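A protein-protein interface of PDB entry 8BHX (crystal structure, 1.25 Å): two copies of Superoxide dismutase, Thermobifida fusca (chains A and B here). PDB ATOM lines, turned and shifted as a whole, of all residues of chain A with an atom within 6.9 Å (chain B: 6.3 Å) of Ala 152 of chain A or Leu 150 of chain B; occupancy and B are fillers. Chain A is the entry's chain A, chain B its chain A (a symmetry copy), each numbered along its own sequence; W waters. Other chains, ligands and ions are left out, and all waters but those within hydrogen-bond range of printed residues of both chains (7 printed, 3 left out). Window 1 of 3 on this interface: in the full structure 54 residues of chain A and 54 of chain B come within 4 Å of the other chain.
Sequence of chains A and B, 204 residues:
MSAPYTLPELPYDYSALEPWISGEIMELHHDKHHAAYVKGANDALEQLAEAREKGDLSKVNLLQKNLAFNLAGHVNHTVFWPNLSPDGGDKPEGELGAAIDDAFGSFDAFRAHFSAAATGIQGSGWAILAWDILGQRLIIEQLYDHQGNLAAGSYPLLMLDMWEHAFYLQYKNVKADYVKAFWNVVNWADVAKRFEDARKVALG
N of Leu 150 of chain B touches CB of Ala 68 of chain A, 3.995 Å away. CD1 of Ile 133 of chain A touches CE1 of Tyr 155 of chain B (3.8 Å). Gln 147 of chain A touches Gly 148 of chain B (O to C, 3.7 Å). Gly 148 of chain A touches Gln 147 of chain B. Leu 150 of chain A touches Ala 152 of chain B (CD1 to CA, 3.7 Å). Ala 151 of chain A touches Ala 72 of chain B (CB to N, 3.96 Å). Pro 156 of chain B touches Leu 203 of chain A.
His 146 of chain A touches none of the printed residues of chain B. Ala 152 of chain A touches just these residues of chain B: Val 75 (3.6 Å) and Leu 150 (3.7 Å). Of the printed residues of chain B, Leu 203 of chain A touches Tyr 155 and Pro 156. Printed residues of chain A within 4 Å of Val 75 of chain B: Leu 134 (3.9 Å) and Ala 152 (3.6 Å). Of the printed residues of chain A, Leu 150 of chain B touches Ala 68, Gln 147, Leu 150 and Ala 152. The nearest residue of chain B that does not touch Ala 152 of chain A is Asn 76 of chain B (4.2 Å). The nearest printed residue of chain B that does not touch Gly 148 of chain A is Gly 148 of chain B (4.2 Å).
Gln 147 of chain A touches Asn 149 of chain B, and with the chains exchanged Asn 149 of chain A touches Gln 147 of chain B. Leu 150 of chain A touches its own counterpart, Leu 150 of chain B. Gly 153 of chain A touches Ser 154 of chain B, and with the chains exchanged Ser 154 of chain A touches Gly 153 of chain B.
Water W4 lies within hydrogen-bond range of O of Ser 154 of chain B (2.7 Å), N of Gly 153 of chain A (2.9 Å) and O of Ala 151 of chain B (3.0 Å). Water W6 lies within hydrogen-bond range of the backbone carbonyl oxygen of Ser 154 of chain A (2.7 Å), the backbone NH of Gly 153 of chain B (2.9 Å) and the backbone carbonyl oxygen of Ala 151 of chain A (3.0 Å).
The backbone NH (N) of Asn 149 of chain A sits at hydrogen-bond distance from the backbone carbonyl oxygen (O) of Gln 147 of chain B (2.9 Å). O of Ser 154 of chain A is in hydrogen-bond range of N of Gly 153 of chain B. The backbone carbonyl oxygen of Ser 154 of chain B is in hydrogen-bond range of the backbone NH of Gly 153 of chain A, at 3.2 Å. The backbone NH (N) of Leu 150 of chain A sits at hydrogen-bond distance from the backbone carbonyl oxygen (O) of Gln 147 of chain B (3.1 Å). O of Gln 147 of chain A lies within hydrogen-bond range of N of Asn 149 of chain B (2.9 Å). The side-chain hydroxyl (OH) of Tyr 155 of chain B is in hydrogen-bond range of the backbone carbonyl oxygen (O) of Leu 203 of chain A (3.1 Å). O of Gln 147 of chain A is in hydrogen-bond range of N of Leu 150 of chain B.
OE1 of Glu 141 of chain B sits at hydrogen-bond distance from OG of Ser 154 of chain B (2.7 Å). The backbone carbonyl oxygen of Gln 142 of chain B is in hydrogen-bond range of the side-chain amide nitrogen of Asn 149 of chain B (2.9 Å). OD1 of Asn 76 of chain B sits close to O of Ala 72 of chain B (3.2 Å). OG of Ser 154 of chain B lies within hydrogen-bond range of O of Ala 151 of chain B (2.7 Å).
Printed residues of chain B that touch a printed residue of chain A: Ala 72, Val 75, Glu 141, Gln 142, Gln 147, Gly 148, Asn 149, Leu 150, Ala 151, Ala 152, Gly 153, Ser 154, Tyr 155 and Pro 156. Of the 20 printed residues of chain A, 15 touch a printed residue of chain B. Hydrophobic or aromatic side chains of chain A that line the printed part of chain B: Ala 68, Leu 71, Ala 72, Ile 133, Leu 134, Leu 150, Ala 151, Ala 152 and Leu 203. Among the printed residues, 24 pairs touch across the chains.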
ATOM      1  N   GLN A  64      32.892   0.338  -6.593  1.00  0.00           N
ATOM      2  CA  GLN A  64      31.762   0.249  -7.511  1.00  0.00           C
ATOM      3  C   GLN A  64      31.743  -1.057  -8.295  1.00  0.00           C
ATOM      4  O   GLN A  64      30.659  -1.511  -8.674  1.00  0.00           O
ATOM      5  CB  GLN A  64      31.731   1.446  -8.452  1.00  0.00           C
ATOM      6  CG  GLN A  64      31.235   2.737  -7.788  1.00  0.00           C
ATOM      7  CD  GLN A  64      29.784   2.662  -7.348  1.00  0.00           C
ATOM      8  OE1 GLN A  64      28.974   1.953  -7.929  1.00  0.00           O
ATOM      9  NE2 GLN A  64      29.461   3.386  -6.309  1.00  0.00           N
ATOM     10  N   ALA A  68      28.625  -3.651  -7.988  1.00  0.00           N
ATOM     11  CA  ALA A  68      27.938  -4.182  -9.161  1.00  0.00           C
ATOM     12  C   ALA A  68      27.998  -5.704  -9.196  1.00  0.00           C
ATOM     13  O   ALA A  68      26.982  -6.365  -9.435  1.00  0.00           O
ATOM     14  CB  ALA A  68      28.565  -3.615 -10.425  1.00  0.00           C
ATOM     15  N   PHE A  69      29.192  -6.270  -8.999  1.00  0.00           N
ATOM     16  CA  PHE A  69      29.354  -7.720  -9.079  1.00  0.00           C
ATOM     17  C   PHE A  69      28.478  -8.440  -8.061  1.00  0.00           C
ATOM     18  O   PHE A  69      27.753  -9.391  -8.397  1.00  0.00           O
ATOM     19  CB  PHE A  69      30.826  -8.084  -8.868  1.00  0.00           C
ATOM     20  CG  PHE A  69      31.074  -9.563  -8.795  1.00  0.00           C
ATOM     21  CD1 PHE A  69      31.006 -10.336  -9.945  1.00  0.00           C
ATOM     22  CD2 PHE A  69      31.356 -10.175  -7.586  1.00  0.00           C
ATOM     23  CE1 PHE A  69      31.227 -11.712  -9.901  1.00  0.00           C
ATOM     24  CE2 PHE A  69      31.577 -11.547  -7.529  1.00  0.00           C
ATOM     25  CZ  PHE A  69      31.506 -12.313  -8.693  1.00  0.00           C
ATOM     26  N   LEU A  71      25.911  -7.146  -6.034  1.00  0.00           N
ATOM     27  CA  LEU A  71      24.480  -6.872  -6.124  1.00  0.00           C
ATOM     28  C   LEU A  71      23.882  -7.582  -7.329  1.00  0.00           C
ATOM     29  O   LEU A  71      22.804  -8.168  -7.241  1.00  0.00           O
ATOM     30  CB  LEU A  71      24.202  -5.366  -6.174  1.00  0.00           C
ATOM     31  CG  LEU A  71      22.724  -4.996  -6.344  1.00  0.00           C
ATOM     32  CD1 LEU A  71      21.865  -5.526  -5.210  1.00  0.00           C
ATOM     33  CD2 LEU A  71      22.554  -3.484  -6.447  1.00  0.00           C
ATOM     34  N   ALA A  72      24.586  -7.579  -8.454  1.00  0.00           N
ATOM     35  CA  ALA A  72      24.102  -8.327  -9.611  1.00  0.00           C
ATOM     36  C   ALA A  72      24.002  -9.815  -9.303  1.00  0.00           C
ATOM     37  O   ALA A  72      23.023 -10.470  -9.679  1.00  0.00           O
ATOM     38  CB  ALA A  72      25.013  -8.074 -10.809  1.00  0.00           C
ATOM     39  N   ASP A 132      12.458  -5.238 -21.884  1.00  0.00           N
ATOM     40  CA  ASP A 132      13.064  -3.929 -22.120  1.00  0.00           C
ATOM     41  C   ASP A 132      12.054  -2.858 -21.749  1.00  0.00           C
ATOM     42  O   ASP A 132      11.004  -2.756 -22.380  1.00  0.00           O
ATOM     43  CB  ASP A 132      13.451  -3.803 -23.590  1.00  0.00           C
ATOM     44  CG  ASP A 132      13.792  -2.380 -23.989  1.00  0.00           C
ATOM     45  OD1 ASP A 132      14.247  -1.603 -23.117  1.00  0.00           O
ATOM     46  OD2 ASP A 132      13.584  -2.060 -25.180  1.00  0.00           O
ATOM     47  N   ILE A 133      12.377  -2.062 -20.721  1.00  0.00           N
ATOM     48  CA  ILE A 133      11.439  -1.044 -20.245  1.00  0.00           C
ATOM     49  C   ILE A 133      11.388   0.210 -21.106  1.00  0.00           C
ATOM     50  O   ILE A 133      10.553   1.078 -20.859  1.00  0.00           O
ATOM     51  CB  ILE A 133      11.673  -0.661 -18.768  1.00  0.00           C
ATOM     52  CG1 ILE A 133      13.023   0.022 -18.556  1.00  0.00           C
ATOM     53  CG2 ILE A 133      11.524  -1.892 -17.883  1.00  0.00           C
ATOM     54  CD1 ILE A 133      13.108   0.748 -17.237  1.00  0.00           C
ATOM     55  N   LEU A 134      12.274   0.344 -22.092  1.00  0.00           N
ATOM     56  CA  LEU A 134      12.158   1.413 -23.079  1.00  0.00           C
ATOM     57  C   LEU A 134      11.244   0.990 -24.225  1.00  0.00           C
ATOM     58  O   LEU A 134      10.180   1.582 -24.438  1.00  0.00           O
ATOM     59  CB  LEU A 134      13.553   1.800 -23.590  1.00  0.00           C
ATOM     60  CG  LEU A 134      13.598   2.851 -24.702  1.00  0.00           C
ATOM     61  CD1 LEU A 134      12.648   3.987 -24.421  1.00  0.00           C
ATOM     62  CD2 LEU A 134      15.025   3.370 -24.856  1.00  0.00           C
ATOM     63  N   GLU A 141      18.966 -11.493 -23.082  1.00  0.00           N
ATOM     64  CA  GLU A 141      20.271 -10.908 -22.826  1.00  0.00           C
ATOM     65  C   GLU A 141      21.226 -12.006 -22.379  1.00  0.00           C
ATOM     66  O   GLU A 141      20.836 -12.925 -21.641  1.00  0.00           O
ATOM     67  CB  GLU A 141      20.192  -9.769 -21.796  1.00  0.00           C
ATOM     68  CG  GLU A 141      19.329  -8.605 -22.300  1.00  0.00           C
ATOM     69  CD  GLU A 141      19.236  -7.444 -21.333  1.00  0.00           C
ATOM     70  OE1 GLU A 141      18.533  -7.553 -20.291  1.00  0.00           O
ATOM     71  OE2 GLU A 141      19.838  -6.394 -21.634  1.00  0.00           O
ATOM     72  N   HIS A 146      28.096 -11.484 -13.684  1.00  0.00           N
ATOM     73  CA  HIS A 146      26.735 -11.168 -13.275  1.00  0.00           C
ATOM     74  C   HIS A 146      26.212  -9.859 -13.830  1.00  0.00           C
ATOM     75  O   HIS A 146      25.000  -9.682 -13.913  1.00  0.00           O
ATOM     76  CB  HIS A 146      26.641 -11.074 -11.744  1.00  0.00           C
ATOM     77  CG  HIS A 146      26.947 -12.353 -11.051  1.00  0.00           C
ATOM     78  ND1 HIS A 146      26.373 -13.542 -11.430  1.00  0.00           N
ATOM     79  CD2 HIS A 146      27.786 -12.633 -10.031  1.00  0.00           C
ATOM     80  CE1 HIS A 146      26.829 -14.502 -10.646  1.00  0.00           C
ATOM     81  NE2 HIS A 146      27.705 -13.983  -9.808  1.00  0.00           N
ATOM     82  N   GLN A 147      27.116  -8.942 -14.168  1.00  0.00           N
ATOM     83  CA  GLN A 147      26.853  -7.510 -14.220  1.00  0.00           C
ATOM     84  C   GLN A 147      27.219  -6.901 -15.562  1.00  0.00           C
ATOM     85  O   GLN A 147      27.285  -5.669 -15.667  1.00  0.00           O
ATOM     86  CB  GLN A 147      27.632  -6.815 -13.084  1.00  0.00           C
ATOM     87  CG  GLN A 147      29.161  -6.711 -13.277  1.00  0.00           C
ATOM     88  CD  GLN A 147      29.987  -7.938 -12.906  1.00  0.00           C
ATOM     89  OE1 GLN A 147      29.482  -9.052 -12.741  1.00  0.00           O
ATOM     90  NE2 GLN A 147      31.288  -7.737 -12.829  1.00  0.00           N
ATOM     91  N   GLY A 148      27.467  -7.711 -16.583  1.00  0.00           N
ATOM     92  CA  GLY A 148      27.883  -7.218 -17.881  1.00  0.00           C
ATOM     93  C   GLY A 148      26.982  -7.627 -19.023  1.00  0.00           C
ATOM     94  O   GLY A 148      26.269  -8.638 -18.945  1.00  0.00           O
ATOM     95  N   ASN A 149      27.034  -6.859 -20.109  1.00  0.00           N
ATOM     96  CA  ASN A 149      26.331  -7.142 -21.358  1.00  0.00           C
ATOM     97  C   ASN A 149      24.818  -7.016 -21.216  1.00  0.00           C
ATOM     98  O   ASN A 149      24.069  -7.859 -21.718  1.00  0.00           O
ATOM     99  CB  ASN A 149      26.732  -8.490 -21.952  1.00  0.00           C
ATOM    100  CG  ASN A 149      26.708  -8.486 -23.463  1.00  0.00           C
ATOM    101  OD1 ASN A 149      27.194  -7.554 -24.125  1.00  0.00           O
ATOM    102  ND2 ASN A 149      26.154  -9.549 -24.033  1.00  0.00           N
ATOM    103  N   LEU A 150      24.360  -5.952 -20.551  1.00  0.00           N
ATOM    104  CA  LEU A 150      22.923  -5.747 -20.383  1.00  0.00           C
ATOM    105  C   LEU A 150      22.592  -4.262 -20.367  1.00  0.00           C
ATOM    106  O   LEU A 150      23.431  -3.398 -20.089  1.00  0.00           O
ATOM    107  CB  LEU A 150      22.370  -6.425 -19.128  1.00  0.00           C
ATOM    108  CG  LEU A 150      22.740  -5.780 -17.796  1.00  0.00           C
ATOM    109  CD1 LEU A 150      21.857  -6.291 -16.684  1.00  0.00           C
ATOM    110  CD2 LEU A 150      24.161  -6.013 -17.458  1.00  0.00           C
ATOM    111  N   ALA A 151      21.337  -3.978 -20.647  1.00  0.00           N
ATOM    112  CA  ALA A 151      20.833  -2.615 -20.709  1.00  0.00           C
ATOM    113  C   ALA A 151      20.181  -2.243 -19.388  1.00  0.00           C
ATOM    114  O   ALA A 151      19.426  -3.026 -18.802  1.00  0.00           O
ATOM    115  CB  ALA A 151      19.795  -2.475 -21.826  1.00  0.00           C
ATOM    116  N   ALA A 152      20.475  -1.036 -18.925  1.00  0.00           N
ATOM    117  CA  ALA A 152      19.875  -0.520 -17.710  1.00  0.00           C
ATOM    118  C   ALA A 152      18.359  -0.583 -17.796  1.00  0.00           C
ATOM    119  O   ALA A 152      17.768  -0.363 -18.858  1.00  0.00           O
ATOM    120  CB  ALA A 152      20.310   0.921 -17.478  1.00  0.00           C
ATOM    121  N   GLY A 153      17.741  -0.896 -16.659  1.00  0.00           N
ATOM    122  CA  GLY A 153      16.309  -0.984 -16.533  1.00  0.00           C
ATOM    123  C   GLY A 153      15.708  -2.290 -16.973  1.00  0.00           C
ATOM    124  O   GLY A 153      14.590  -2.603 -16.558  1.00  0.00           O
ATOM    125  N   SER A 154      16.406  -3.072 -17.796  1.00  0.00           N
ATOM    126  CA  SER A 154      15.787  -4.279 -18.324  1.00  0.00           C
ATOM    127  C   SER A 154      15.443  -5.205 -17.164  1.00  0.00           C
ATOM    128  O   SER A 154      16.229  -5.381 -16.229  1.00  0.00           O
ATOM    129  CB  SER A 154      16.660  -4.940 -19.399  1.00  0.00           C
ATOM    130  OG  SER A 154      17.943  -5.310 -18.954  1.00  0.00           O
ATOM    131  N   TYR A 155      14.225  -5.732 -17.195  1.00  0.00           N
ATOM    132  CA  TYR A 155      13.627  -6.354 -16.016  1.00  0.00           C
ATOM    133  C   TYR A 155      13.686  -7.868 -16.162  1.00  0.00           C
ATOM    134  O   TYR A 155      13.081  -8.414 -17.096  1.00  0.00           O
ATOM    135  CB  TYR A 155      12.191  -5.867 -15.882  1.00  0.00           C
ATOM    136  CG  TYR A 155      11.486  -6.233 -14.597  1.00  0.00           C
ATOM    137  CD1 TYR A 155      11.316  -5.309 -13.585  1.00  0.00           C
ATOM    138  CD2 TYR A 155      10.960  -7.498 -14.412  1.00  0.00           C
ATOM    139  CE1 TYR A 155      10.656  -5.644 -12.412  1.00  0.00           C
ATOM    140  CE2 TYR A 155      10.288  -7.841 -13.239  1.00  0.00           C
ATOM    141  CZ  TYR A 155      10.142  -6.913 -12.251  1.00  0.00           C
ATOM    142  OH  TYR A 155       9.478  -7.280 -11.098  1.00  0.00           O
ATOM    143  N   LEU A 203      10.599   3.205 -18.938  1.00  0.00           N
ATOM    144  CA  LEU A 203      11.778   4.028 -18.700  1.00  0.00           C
ATOM    145  C   LEU A 203      11.409   5.476 -18.442  1.00  0.00           C
ATOM    146  O   LEU A 203      11.981   6.118 -17.613  1.00  0.00           O
ATOM    147  CB  LEU A 203      12.725   3.964 -19.889  1.00  0.00           C
ATOM    148  CG  LEU A 203      14.107   4.633 -19.718  1.00  0.00           C
ATOM    149  CD1 LEU A 203      14.970   3.916 -18.665  1.00  0.00           C
ATOM    150  CD2 LEU A 203      14.824   4.682 -21.041  1.00  0.00           C
ATOM    151  N   ALA B  72      21.624  -0.465 -24.703  1.00  0.00           N
ATOM    152  CA  ALA B  72      22.108   0.283 -23.546  1.00  0.00           C
ATOM    153  C   ALA B  72      22.455   1.717 -23.922  1.00  0.00           C
ATOM    154  O   ALA B  72      22.132   2.656 -23.184  1.00  0.00           O
ATOM    155  CB  ALA B  72      23.312  -0.430 -22.934  1.00  0.00           C
ATOM    156  N   VAL B  75      19.081   3.511 -24.264  1.00  0.00           N
ATOM    157  CA  VAL B  75      18.515   3.756 -22.939  1.00  0.00           C
ATOM    158  C   VAL B  75      19.249   4.895 -22.246  1.00  0.00           C
ATOM    159  O   VAL B  75      18.633   5.818 -21.693  1.00  0.00           O
ATOM    160  CB  VAL B  75      18.576   2.465 -22.099  1.00  0.00           C
ATOM    161  CG1 VAL B  75      18.363   2.767 -20.634  1.00  0.00           C
ATOM    162  CG2 VAL B  75      17.559   1.442 -22.579  1.00  0.00           C
ATOM    163  N   ASN B  76      20.576   4.815 -22.219  1.00  0.00           N
ATOM    164  CA  ASN B  76      21.354   5.744 -21.422  1.00  0.00           C
ATOM    165  C   ASN B  76      21.183   7.176 -21.935  1.00  0.00           C
ATOM    166  O   ASN B  76      21.014   8.116 -21.144  1.00  0.00           O
ATOM    167  CB  ASN B  76      22.836   5.359 -21.444  1.00  0.00           C
ATOM    168  CG  ASN B  76      23.142   4.050 -20.744  1.00  0.00           C
ATOM    169  OD1 ASN B  76      22.306   3.476 -20.069  1.00  0.00           O
ATOM    170  ND2 ASN B  76      24.365   3.589 -20.907  1.00  0.00           N
ATOM    171  N   ILE B 128      26.136   7.020 -12.820  1.00  0.00           N
ATOM    172  CA  ILE B 128      24.685   7.122 -12.737  1.00  0.00           C
ATOM    173  C   ILE B 128      24.231   6.987 -11.290  1.00  0.00           C
ATOM    174  O   ILE B 128      24.879   6.323 -10.461  1.00  0.00           O
ATOM    175  CB  ILE B 128      23.913   6.112 -13.622  1.00  0.00           C
ATOM    176  CG1 ILE B 128      23.889   4.697 -13.031  1.00  0.00           C
ATOM    177  CG2 ILE B 128      24.575   6.029 -14.977  1.00  0.00           C
ATOM    178  CD1 ILE B 128      22.916   3.750 -13.783  1.00  0.00           C
ATOM    179  N   GLU B 141      25.988   3.723  -9.726  1.00  0.00           N
ATOM    180  CA  GLU B 141      26.651   2.709 -10.528  1.00  0.00           C
ATOM    181  C   GLU B 141      27.599   3.393 -11.504  1.00  0.00           C
ATOM    182  O   GLU B 141      27.287   4.464 -12.047  1.00  0.00           O
ATOM    183  CB  GLU B 141      25.640   1.808 -11.256  1.00  0.00           C
ATOM    184  CG  GLU B 141      24.766   1.022 -10.269  1.00  0.00           C
ATOM    185  CD  GLU B 141      23.767   0.099 -10.933  1.00  0.00           C
ATOM    186  OE1 GLU B 141      22.747   0.583 -11.497  1.00  0.00           O
ATOM    187  OE2 GLU B 141      23.977  -1.128 -10.857  1.00  0.00           O
ATOM    188  N   GLN B 142      28.780   2.811 -11.690  1.00  0.00           N
ATOM    189  CA  GLN B 142      29.778   3.310 -12.635  1.00  0.00           C
ATOM    190  C   GLN B 142      29.744   2.366 -13.835  1.00  0.00           C
ATOM    191  O   GLN B 142      30.292   1.258 -13.772  1.00  0.00           O
ATOM    192  CB  GLN B 142      31.152   3.335 -11.974  1.00  0.00           C
ATOM    193  CG  GLN B 142      32.226   3.921 -12.860  1.00  0.00           C
ATOM    194  CD  GLN B 142      33.615   3.683 -12.314  1.00  0.00           C
ATOM    195  OE1 GLN B 142      34.071   2.533 -12.222  1.00  0.00           O
ATOM    196  NE2 GLN B 142      34.313   4.757 -11.962  1.00  0.00           N
ATOM    197  N   LEU B 143      29.074   2.770 -14.904  1.00  0.00           N
ATOM    198  CA  LEU B 143      28.901   1.900 -16.058  1.00  0.00           C
ATOM    199  C   LEU B 143      30.155   1.905 -16.909  1.00  0.00           C
ATOM    200  O   LEU B 143      30.795   2.950 -17.087  1.00  0.00           O
ATOM    201  CB  LEU B 143      27.732   2.352 -16.927  1.00  0.00           C
ATOM    202  CG  LEU B 143      26.391   2.591 -16.247  1.00  0.00           C
ATOM    203  CD1 LEU B 143      25.331   2.911 -17.286  1.00  0.00           C
ATOM    204  CD2 LEU B 143      26.005   1.382 -15.437  1.00  0.00           C
ATOM    205  N   HIS B 146      28.452   1.189 -22.343  1.00  0.00           N
ATOM    206  CA  HIS B 146      27.068   1.470 -21.990  1.00  0.00           C
ATOM    207  C   HIS B 146      26.428   0.414 -21.111  1.00  0.00           C
ATOM    208  O   HIS B 146      25.456   0.713 -20.423  1.00  0.00           O
ATOM    209  CB  HIS B 146      26.203   1.585 -23.254  1.00  0.00           C
ATOM    210  CG  HIS B 146      26.594   2.712 -24.141  1.00  0.00           C
ATOM    211  ND1 HIS B 146      26.795   3.983 -23.659  1.00  0.00           N
ATOM    212  CD2 HIS B 146      26.852   2.754 -25.465  1.00  0.00           C
ATOM    213  CE1 HIS B 146      27.135   4.769 -24.663  1.00  0.00           C
ATOM    214  NE2 HIS B 146      27.202   4.045 -25.763  1.00  0.00           N
ATOM    215  N   GLN B 147      26.944  -0.812 -21.168  1.00  0.00           N
ATOM    216  CA  GLN B 147      26.209  -2.027 -20.839  1.00  0.00           C
ATOM    217  C   GLN B 147      26.921  -2.870 -19.797  1.00  0.00           C
ATOM    218  O   GLN B 147      26.547  -4.035 -19.606  1.00  0.00           O
ATOM    219  CB  GLN B 147      25.986  -2.842 -22.129  1.00  0.00           C
ATOM    220  CG  GLN B 147      27.231  -3.551 -22.707  1.00  0.00           C
ATOM    221  CD  GLN B 147      28.166  -2.707 -23.566  1.00  0.00           C
ATOM    222  OE1 GLN B 147      28.123  -1.474 -23.580  1.00  0.00           O
ATOM    223  NE2 GLN B 147      29.064  -3.387 -24.254  1.00  0.00           N
ATOM    224  N   GLY B 148      27.932  -2.334 -19.125  1.00  0.00           N
ATOM    225  CA  GLY B 148      28.706  -3.087 -18.158  1.00  0.00           C
ATOM    226  C   GLY B 148      28.727  -2.486 -16.770  1.00  0.00           C
ATOM    227  O   GLY B 148      28.525  -1.276 -16.595  1.00  0.00           O
ATOM    228  N   ASN B 149      29.006  -3.327 -15.777  1.00  0.00           N
ATOM    229  CA  ASN B 149      29.185  -2.929 -14.382  1.00  0.00           C
ATOM    230  C   ASN B 149      27.888  -2.442 -13.744  1.00  0.00           C
ATOM    231  O   ASN B 149      27.880  -1.435 -13.032  1.00  0.00           O
ATOM    232  CB  ASN B 149      30.313  -1.914 -14.213  1.00  0.00           C
ATOM    233  CG  ASN B 149      31.039  -2.071 -12.897  1.00  0.00           C
ATOM    234  OD1 ASN B 149      31.383  -3.184 -12.466  1.00  0.00           O
ATOM    235  ND2 ASN B 149      31.301  -0.944 -12.245  1.00  0.00           N
ATOM    236  N   LEU B 150      26.792  -3.168 -13.977  1.00  0.00           N
ATOM    237  CA  LEU B 150      25.511  -2.781 -13.391  1.00  0.00           C
ATOM    238  C   LEU B 150      24.669  -4.011 -13.082  1.00  0.00           C
ATOM    239  O   LEU B 150      24.851  -5.097 -13.643  1.00  0.00           O
ATOM    240  CB  LEU B 150      24.723  -1.811 -14.274  1.00  0.00           C
ATOM    241  CG  LEU B 150      24.103  -2.402 -15.536  1.00  0.00           C
ATOM    242  CD1 LEU B 150      23.065  -1.472 -16.115  1.00  0.00           C
ATOM    243  CD2 LEU B 150      25.133  -2.703 -16.555  1.00  0.00           C
ATOM    244  N   ALA B 151      23.721  -3.815 -12.190  1.00  0.00           N
ATOM    245  CA  ALA B 151      22.831  -4.875 -11.741  1.00  0.00           C
ATOM    246  C   ALA B 151      21.527  -4.820 -12.519  1.00  0.00           C
ATOM    247  O   ALA B 151      20.953  -3.748 -12.736  1.00  0.00           O
ATOM    248  CB  ALA B 151      22.520  -4.721 -10.249  1.00  0.00           C
ATOM    249  N   ALA B 152      21.060  -5.990 -12.933  1.00  0.00           N
ATOM    250  CA  ALA B 152      19.793  -6.100 -13.631  1.00  0.00           C
ATOM    251  C   ALA B 152      18.680  -5.463 -12.814  1.00  0.00           C
ATOM    252  O   ALA B 152      18.658  -5.550 -11.582  1.00  0.00           O
ATOM    253  CB  ALA B 152      19.458  -7.562 -13.890  1.00  0.00           C
ATOM    254  N   GLY B 153      17.757  -4.815 -13.524  1.00  0.00           N
ATOM    255  CA  GLY B 153      16.615  -4.166 -12.935  1.00  0.00           C
ATOM    256  C   GLY B 153      16.870  -2.785 -12.399  1.00  0.00           C
ATOM    257  O   GLY B 153      15.916  -2.021 -12.238  1.00  0.00           O
ATOM    258  N   SER B 154      18.123  -2.428 -12.117  1.00  0.00           N
ATOM    259  CA  SER B 154      18.370  -1.139 -11.486  1.00  0.00           C
ATOM    260  C   SER B 154      17.888  -0.034 -12.417  1.00  0.00           C
ATOM    261  O   SER B 154      18.106  -0.077 -13.630  1.00  0.00           O
ATOM    262  CB  SER B 154      19.836  -0.988 -11.060  1.00  0.00           C
ATOM    263  OG  SER B 154      20.758  -1.098 -12.118  1.00  0.00           O
ATOM    264  N   TYR B 155      17.158   0.917 -11.845  1.00  0.00           N
ATOM    265  CA  TYR B 155      16.352   1.845 -12.635  1.00  0.00           C
ATOM    266  C   TYR B 155      17.056   3.193 -12.700  1.00  0.00           C
ATOM    267  O   TYR B 155      17.258   3.827 -11.654  1.00  0.00           O
ATOM    268  CB  TYR B 155      14.979   1.970 -11.988  1.00  0.00           C
ATOM    269  CG  TYR B 155      13.937   2.716 -12.788  1.00  0.00           C
ATOM    270  CD1 TYR B 155      12.947   2.045 -13.478  1.00  0.00           C
ATOM    271  CD2 TYR B 155      13.927   4.098 -12.825  1.00  0.00           C
ATOM    272  CE1 TYR B 155      11.984   2.734 -14.200  1.00  0.00           C
ATOM    273  CE2 TYR B 155      12.957   4.799 -13.541  1.00  0.00           C
ATOM    274  CZ  TYR B 155      11.996   4.112 -14.222  1.00  0.00           C
ATOM    275  OH  TYR B 155      11.052   4.829 -14.929  1.00  0.00           O
ATOM    276  N   PRO B 156      17.437   3.674 -13.879  1.00  0.00           N
ATOM    277  CA  PRO B 156      18.251   4.896 -13.947  1.00  0.00           C
ATOM    278  C   PRO B 156      17.478   6.160 -13.596  1.00  0.00           C
ATOM    279  O   PRO B 156      16.348   6.365 -14.034  1.00  0.00           O
ATOM    280  CB  PRO B 156      18.725   4.924 -15.406  1.00  0.00           C
ATOM    281  CG  PRO B 156      17.739   4.093 -16.156  1.00  0.00           C
ATOM    282  CD  PRO B 156      17.178   3.091 -15.204  1.00  0.00           C
ATOM    283  N   MET B 159      22.006  10.429 -15.136  1.00  0.00           N
ATOM    284  CA  MET B 159      23.113   9.931 -15.938  1.00  0.00           C
ATOM    285  C   MET B 159      24.136  11.034 -16.173  1.00  0.00           C
ATOM    286  O   MET B 159      23.764  12.189 -16.409  1.00  0.00           O
ATOM    287  CB  MET B 159      22.615   9.555 -17.333  1.00  0.00           C
ATOM    288  CG  MET B 159      21.388   8.663 -17.380  1.00  0.00           C
ATOM    289  SD  MET B 159      21.614   7.020 -16.705  1.00  0.00           S
ATOM    290  CE  MET B 159      22.684   6.288 -17.943  1.00  0.00           C
HETATM  291  O   HOH W   1      22.468  -8.461 -13.057  1.00  0.00           O
HETATM  292  O   HOH W   2      32.209  -5.189 -14.042  1.00  0.00           O
HETATM  293  O   HOH W   3      29.392  -6.207 -23.388  1.00  0.00           O
HETATM  294  O   HOH W   4      19.688  -1.894 -14.768  1.00  0.00           O
HETATM  295  O   HOH W   5      10.748   7.782 -15.331  1.00  0.00           O
HETATM  296  O   HOH W   6      18.726  -4.452 -16.224  1.00  0.00           O
HETATM  297  O   HOH W   7      22.590   0.667 -19.780  1.00  0.00           O
